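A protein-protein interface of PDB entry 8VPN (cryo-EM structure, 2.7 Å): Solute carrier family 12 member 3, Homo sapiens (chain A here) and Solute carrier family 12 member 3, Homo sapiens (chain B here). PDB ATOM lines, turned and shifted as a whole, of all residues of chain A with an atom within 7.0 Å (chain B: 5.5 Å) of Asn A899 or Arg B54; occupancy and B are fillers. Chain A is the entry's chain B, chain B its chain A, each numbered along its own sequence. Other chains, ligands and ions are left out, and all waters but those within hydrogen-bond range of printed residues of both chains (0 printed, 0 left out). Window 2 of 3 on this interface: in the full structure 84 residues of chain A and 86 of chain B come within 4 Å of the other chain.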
ATOM      1  N   GLY A 866      24.446  29.336 -12.729  1.00  0.00           N
ATOM      2  CA  GLY A 866      24.596  30.743 -12.425  1.00  0.00           C
ATOM      3  C   GLY A 866      24.248  31.123 -11.001  1.00  0.00           C
ATOM      4  O   GLY A 866      24.633  30.436 -10.049  1.00  0.00           O
ATOM      5  N   GLN A 867      23.536  32.233 -10.845  1.00  0.00           N
ATOM      6  CA  GLN A 867      23.109  32.719  -9.543  1.00  0.00           C
ATOM      7  C   GLN A 867      21.623  33.043  -9.586  1.00  0.00           C
ATOM      8  O   GLN A 867      21.040  33.246 -10.654  1.00  0.00           O
ATOM      9  CB  GLN A 867      23.909  33.955  -9.115  1.00  0.00           C
ATOM     10  CG  GLN A 867      24.337  33.939  -7.662  1.00  0.00           C
ATOM     11  CD  GLN A 867      23.209  34.327  -6.726  1.00  0.00           C
ATOM     12  OE1 GLN A 867      22.570  35.363  -6.903  1.00  0.00           O
ATOM     13  NE2 GLN A 867      22.951  33.489  -5.731  1.00  0.00           N
ATOM     14  N   ILE A 868      21.009  33.088  -8.404  1.00  0.00           N
ATOM     15  CA  ILE A 868      19.590  33.410  -8.313  1.00  0.00           C
ATOM     16  C   ILE A 868      19.321  34.912  -8.299  1.00  0.00           C
ATOM     17  O   ILE A 868      18.221  35.337  -8.678  1.00  0.00           O
ATOM     18  CB  ILE A 868      18.965  32.757  -7.066  1.00  0.00           C
ATOM     19  CG1 ILE A 868      17.537  33.258  -6.856  1.00  0.00           C
ATOM     20  CG2 ILE A 868      19.817  33.033  -5.841  1.00  0.00           C
ATOM     21  CD1 ILE A 868      16.634  33.047  -8.047  1.00  0.00           C
ATOM     22  N   ARG A 870      21.290  37.179  -9.980  1.00  0.00           N
ATOM     23  CA  ARG A 870      21.859  37.788 -11.177  1.00  0.00           C
ATOM     24  C   ARG A 870      21.470  37.009 -12.425  1.00  0.00           C
ATOM     25  O   ARG A 870      22.225  36.975 -13.403  1.00  0.00           O
ATOM     26  CB  ARG A 870      23.382  37.883 -11.081  1.00  0.00           C
ATOM     27  CG  ARG A 870      23.901  38.367  -9.736  1.00  0.00           C
ATOM     28  CD  ARG A 870      25.404  38.590  -9.791  1.00  0.00           C
ATOM     29  NE  ARG A 870      26.130  37.328  -9.851  1.00  0.00           N
ATOM     30  CZ  ARG A 870      27.058  36.952  -8.982  1.00  0.00           C
ATOM     31  NH1 ARG A 870      27.415  37.727  -7.973  1.00  0.00           N
ATOM     32  NH2 ARG A 870      27.644  35.768  -9.131  1.00  0.00           N
ATOM     33  N   PRO A 896      20.054  28.040 -11.246  1.00  0.00           N
ATOM     34  CA  PRO A 896      20.614  28.652 -10.030  1.00  0.00           C
ATOM     35  C   PRO A 896      20.592  27.780  -8.777  1.00  0.00           C
ATOM     36  O   PRO A 896      20.934  28.292  -7.706  1.00  0.00           O
ATOM     37  CB  PRO A 896      19.698  29.866  -9.844  1.00  0.00           C
ATOM     38  CG  PRO A 896      18.363  29.403 -10.359  1.00  0.00           C
ATOM     39  CD  PRO A 896      18.608  28.286 -11.360  1.00  0.00           C
ATOM     40  N   ASP A 897      20.214  26.507  -8.869  1.00  0.00           N
ATOM     41  CA  ASP A 897      20.039  25.664  -7.687  1.00  0.00           C
ATOM     42  C   ASP A 897      20.790  24.345  -7.842  1.00  0.00           C
ATOM     43  O   ASP A 897      20.273  23.265  -7.556  1.00  0.00           O
ATOM     44  CB  ASP A 897      18.554  25.430  -7.408  1.00  0.00           C
ATOM     45  CG  ASP A 897      17.852  24.700  -8.534  1.00  0.00           C
ATOM     46  OD1 ASP A 897      18.014  23.469  -8.640  1.00  0.00           O
ATOM     47  OD2 ASP A 897      17.131  25.356  -9.312  1.00  0.00           O
ATOM     48  N   ILE A 898      22.047  24.421  -8.286  1.00  0.00           N
ATOM     49  CA  ILE A 898      22.864  23.215  -8.426  1.00  0.00           C
ATOM     50  C   ILE A 898      23.610  22.855  -7.152  1.00  0.00           C
ATOM     51  O   ILE A 898      24.177  21.759  -7.064  1.00  0.00           O
ATOM     52  CB  ILE A 898      23.866  23.381  -9.585  1.00  0.00           C
ATOM     53  CG1 ILE A 898      23.119  23.611 -10.896  1.00  0.00           C
ATOM     54  CG2 ILE A 898      24.761  22.161  -9.712  1.00  0.00           C
ATOM     55  CD1 ILE A 898      23.943  23.311 -12.113  1.00  0.00           C
ATOM     56  N   ASN A 899      23.623  23.741  -6.159  1.00  0.00           N
ATOM     57  CA  ASN A 899      24.274  23.479  -4.883  1.00  0.00           C
ATOM     58  C   ASN A 899      23.315  22.959  -3.822  1.00  0.00           C
ATOM     59  O   ASN A 899      23.761  22.596  -2.731  1.00  0.00           O
ATOM     60  CB  ASN A 899      24.950  24.752  -4.366  1.00  0.00           C
ATOM     61  CG  ASN A 899      26.212  25.094  -5.128  1.00  0.00           C
ATOM     62  OD1 ASN A 899      27.095  24.257  -5.303  1.00  0.00           O
ATOM     63  ND2 ASN A 899      26.302  26.334  -5.588  1.00  0.00           N
ATOM     64  N   GLN A 900      22.020  22.916  -4.114  1.00  0.00           N
ATOM     65  CA  GLN A 900      21.025  22.542  -3.125  1.00  0.00           C
ATOM     66  C   GLN A 900      21.161  21.067  -2.751  1.00  0.00           C
ATOM     67  O   GLN A 900      21.734  20.260  -3.483  1.00  0.00           O
ATOM     68  CB  GLN A 900      19.626  22.845  -3.659  1.00  0.00           C
ATOM     69  CG  GLN A 900      18.526  21.945  -3.152  1.00  0.00           C
ATOM     70  CD  GLN A 900      17.166  22.361  -3.670  1.00  0.00           C
ATOM     71  OE1 GLN A 900      16.437  21.562  -4.258  1.00  0.00           O
ATOM     72  NE2 GLN A 900      16.822  23.624  -3.465  1.00  0.00           N
ATOM     73  N   ASN A 901      20.629  20.725  -1.583  1.00  0.00           N
ATOM     74  CA  ASN A 901      20.741  19.369  -1.073  1.00  0.00           C
ATOM     75  C   ASN A 901      19.921  18.399  -1.922  1.00  0.00           C
ATOM     76  O   ASN A 901      18.772  18.694  -2.269  1.00  0.00           O
ATOM     77  CB  ASN A 901      20.261  19.313   0.375  1.00  0.00           C
ATOM     78  CG  ASN A 901      21.009  18.295   1.198  1.00  0.00           C
ATOM     79  OD1 ASN A 901      21.879  17.588   0.693  1.00  0.00           O
ATOM     80  ND2 ASN A 901      20.669  18.208   2.476  1.00  0.00           N
ATOM     81  N   PRO A 902      20.474  17.240  -2.267  1.00  0.00           N
ATOM     82  CA  PRO A 902      19.690  16.234  -2.988  1.00  0.00           C
ATOM     83  C   PRO A 902      18.616  15.626  -2.101  1.00  0.00           C
ATOM     84  O   PRO A 902      18.597  15.802  -0.882  1.00  0.00           O
ATOM     85  CB  PRO A 902      20.733  15.188  -3.390  1.00  0.00           C
ATOM     86  CG  PRO A 902      21.841  15.373  -2.420  1.00  0.00           C
ATOM     87  CD  PRO A 902      21.879  16.833  -2.104  1.00  0.00           C
ATOM     88  N   VAL A 950      31.491  16.410  -0.680  1.00  0.00           N
ATOM     89  CA  VAL A 950      30.791  17.495  -1.365  1.00  0.00           C
ATOM     90  C   VAL A 950      30.649  17.184  -2.849  1.00  0.00           C
ATOM     91  O   VAL A 950      29.564  17.316  -3.428  1.00  0.00           O
ATOM     92  CB  VAL A 950      31.530  18.825  -1.141  1.00  0.00           C
ATOM     93  CG1 VAL A 950      30.633  19.996  -1.486  1.00  0.00           C
ATOM     94  CG2 VAL A 950      32.028  18.916   0.290  1.00  0.00           C
ATOM     95  N   ARG A 954      27.075  16.805  -5.468  1.00  0.00           N
ATOM     96  CA  ARG A 954      26.777  17.566  -6.674  1.00  0.00           C
ATOM     97  C   ARG A 954      26.596  16.657  -7.879  1.00  0.00           C
ATOM     98  O   ARG A 954      25.933  17.047  -8.845  1.00  0.00           O
ATOM     99  CB  ARG A 954      27.882  18.585  -6.948  1.00  0.00           C
ATOM    100  CG  ARG A 954      27.693  19.367  -8.230  1.00  0.00           C
ATOM    101  CD  ARG A 954      28.955  20.115  -8.616  1.00  0.00           C
ATOM    102  NE  ARG A 954      29.705  20.562  -7.449  1.00  0.00           N
ATOM    103  CZ  ARG A 954      31.008  20.382  -7.284  1.00  0.00           C
ATOM    104  NH1 ARG A 954      31.738  19.750  -8.187  1.00  0.00           N
ATOM    105  NH2 ARG A 954      31.593  20.846  -6.183  1.00  0.00           N
ATOM    106  N   ARG A 957      22.879  15.235  -7.552  1.00  0.00           N
ATOM    107  CA  ARG A 957      21.895  16.301  -7.694  1.00  0.00           C
ATOM    108  C   ARG A 957      21.687  16.660  -9.159  1.00  0.00           C
ATOM    109  O   ARG A 957      20.574  17.008  -9.569  1.00  0.00           O
ATOM    110  CB  ARG A 957      22.331  17.526  -6.894  1.00  0.00           C
ATOM    111  CG  ARG A 957      21.635  18.812  -7.293  1.00  0.00           C
ATOM    112  CD  ARG A 957      20.154  18.791  -6.968  1.00  0.00           C
ATOM    113  NE  ARG A 957      19.641  20.147  -6.835  1.00  0.00           N
ATOM    114  CZ  ARG A 957      18.461  20.558  -7.276  1.00  0.00           C
ATOM    115  NH1 ARG A 957      17.602  19.723  -7.836  1.00  0.00           N
ATOM    116  NH2 ARG A 957      18.136  21.841  -7.154  1.00  0.00           N
ATOM    117  N   CYS B  52      24.654  26.864  -0.105  1.00  0.00           N
ATOM    118  CA  CYS B  52      23.764  28.019  -0.060  1.00  0.00           C
ATOM    119  C   CYS B  52      23.758  28.756  -1.398  1.00  0.00           C
ATOM    120  O   CYS B  52      24.248  28.240  -2.401  1.00  0.00           O
ATOM    121  CB  CYS B  52      24.175  28.969   1.066  1.00  0.00           C
ATOM    122  SG  CYS B  52      23.063  30.380   1.290  1.00  0.00           S
ATOM    123  N   MET B  53      23.204  29.969  -1.405  1.00  0.00           N
ATOM    124  CA  MET B  53      23.081  30.764  -2.627  1.00  0.00           C
ATOM    125  C   MET B  53      24.409  31.464  -2.927  1.00  0.00           C
ATOM    126  O   MET B  53      24.635  32.630  -2.593  1.00  0.00           O
ATOM    127  CB  MET B  53      21.940  31.763  -2.500  1.00  0.00           C
ATOM    128  N   ARG B  54      25.307  30.702  -3.556  1.00  0.00           N
ATOM    129  CA  ARG B  54      26.616  31.268  -3.967  1.00  0.00           C
ATOM    130  C   ARG B  54      26.890  30.812  -5.403  1.00  0.00           C
ATOM    131  O   ARG B  54      26.480  29.694  -5.749  1.00  0.00           O
ATOM    132  CB  ARG B  54      27.728  30.831  -3.013  1.00  0.00           C
ATOM    133  CG  ARG B  54      27.553  31.307  -1.579  1.00  0.00           C
ATOM    134  CD  ARG B  54      28.887  31.270  -0.864  1.00  0.00           C
ATOM    135  NE  ARG B  54      29.893  31.935  -1.678  1.00  0.00           N
ATOM    136  CZ  ARG B  54      31.170  32.058  -1.345  1.00  0.00           C
ATOM    137  NH1 ARG B  54      31.604  31.559  -0.202  1.00  0.00           N
ATOM    138  NH2 ARG B  54      32.006  32.681  -2.155  1.00  0.00           N
ATOM    139  N   TPO B  55      27.546  31.649  -6.200  1.00  0.00           N
ATOM    140  CA  TPO B  55      27.829  31.339  -7.626  1.00  0.00           C
ATOM    141  CB  TPO B  55      28.933  32.265  -8.158  1.00  0.00           C
ATOM    142  CG2 TPO B  55      28.922  32.368  -9.666  1.00  0.00           C
ATOM    143  OG1 TPO B  55      28.725  33.616  -7.617  1.00  0.00           O
ATOM    144  P   TPO B  55      29.261  34.056  -6.157  1.00  0.00           P
ATOM    145  O1P TPO B  55      30.315  33.032  -5.794  1.00  0.00           O
ATOM    146  O2P TPO B  55      28.059  34.008  -5.237  1.00  0.00           O
ATOM    147  O3P TPO B  55      29.827  35.455  -6.316  1.00  0.00           O
ATOM    148  C   TPO B  55      28.267  29.886  -7.818  1.00  0.00           C
ATOM    149  O   TPO B  55      28.995  29.376  -6.953  1.00  0.00           O
ATOM    150  N   PHE B  56      27.861  29.254  -8.921  1.00  0.00           N
ATOM    151  CA  PHE B  56      28.362  27.895  -9.235  1.00  0.00           C
ATOM    152  C   PHE B  56      29.849  27.995  -9.569  1.00  0.00           C
ATOM    153  O   PHE B  56      30.197  28.758 -10.484  1.00  0.00           O
ATOM    154  CB  PHE B  56      27.628  27.322 -10.444  1.00  0.00           C
ATOM    155  CG  PHE B  56      28.059  25.935 -10.845  1.00  0.00           C
ATOM    156  CD1 PHE B  56      27.950  24.874  -9.962  1.00  0.00           C
ATOM    157  CD2 PHE B  56      28.566  25.688 -12.111  1.00  0.00           C
ATOM    158  CE1 PHE B  56      28.349  23.601 -10.331  1.00  0.00           C
ATOM    159  CE2 PHE B  56      28.963  24.412 -12.480  1.00  0.00           C
ATOM    160  CZ  PHE B  56      28.854  23.372 -11.588  1.00  0.00           C
ATOM    161  N   TYR B  58      32.507  28.169  -6.919  1.00  0.00           N
ATOM    162  CA  TYR B  58      33.338  28.727  -5.861  1.00  0.00           C
ATOM    163  C   TYR B  58      34.015  27.672  -4.994  1.00  0.00           C
ATOM    164  O   TYR B  58      34.946  28.013  -4.257  1.00  0.00           O
ATOM    165  CB  TYR B  58      32.498  29.651  -4.972  1.00  0.00           C
ATOM    166  CG  TYR B  58      31.749  28.931  -3.873  1.00  0.00           C
ATOM    167  CD1 TYR B  58      32.216  28.933  -2.566  1.00  0.00           C
ATOM    168  CD2 TYR B  58      30.572  28.249  -4.144  1.00  0.00           C
ATOM    169  CE1 TYR B  58      31.533  28.271  -1.565  1.00  0.00           C
ATOM    170  CE2 TYR B  58      29.886  27.590  -3.152  1.00  0.00           C
ATOM    171  CZ  TYR B  58      30.367  27.601  -1.866  1.00  0.00           C
ATOM    172  OH  TYR B  58      29.674  26.938  -0.880  1.00  0.00           O
ATOM    173  N   ASN B  59      33.594  26.415  -5.069  1.00  0.00           N
ATOM    174  CA  ASN B  59      34.091  25.398  -4.147  1.00  0.00           C
ATOM    175  C   ASN B  59      34.996  24.367  -4.814  1.00  0.00           C
ATOM    176  O   ASN B  59      35.405  23.397  -4.177  1.00  0.00           O
ATOM    177  CB  ASN B  59      32.919  24.684  -3.472  1.00  0.00           C
ATOM    178  CG  ASN B  59      31.823  24.320  -4.448  1.00  0.00           C
ATOM    179  OD1 ASN B  59      31.912  24.624  -5.634  1.00  0.00           O
ATOM    180  ND2 ASN B  59      30.778  23.667  -3.954  1.00  0.00           N
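O of Arg B54 is in hydrogen-bond range of ND2 of Asn A899 (3.4 Å).
O3P of TPO B55 lies close to NH2 of Arg A870, 3.6 Å away.
O of Gly A866 touches N of Phe B56, 3.6 Å away.
O of Met B53 touches NE2 of Gln A867 (3.7 Å).
Phe B56 touches Ile A898.
Asn A899 touches Asn B59 (OD1 to ND2, 3.97 Å).
Phe B56 touches Arg A954.
Asn B59 touches Arg A954 (ND2 to NH2, 3.7 Å).
Of the printed residues of chain B, Asn A899 touches Arg B54 and Asn B59.
Arg B54 touches just one residue of chain A: Asn A899.
Printed residues of chain B within 4 Å of Arg A954: Phe B56 and Asn B59.
Of the printed residues of chain B, Gly A866 touches Phe B56.
Printed residues of chain B within 4 Å of Ile A898: Phe B56.
Of the printed residues of chain B, Arg A870 touches TPO B55 (2.8 Å).
Asn A901 touches none of the printed residues of chain B.
Tyr B58 touches none of the printed residues of chain A.
The nearest printed residue of chain A that does not touch Asn B59 is Val A950 (4.4 Å).
Hydrophobic or aromatic side chains of chain B within 4 Å of the printed part of chain A: Met B53 and Phe B56.
Hydrophobic or aromatic side chains of chain A within 4 Å of the printed part of chain B: Ile A898.
Among the printed residues, 8 pairs touch across the chains.
Among the printed residues, no Asp or Glu carboxylate lies within 4 Å of a Lys or Arg side-chain nitrogen of the other chain.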
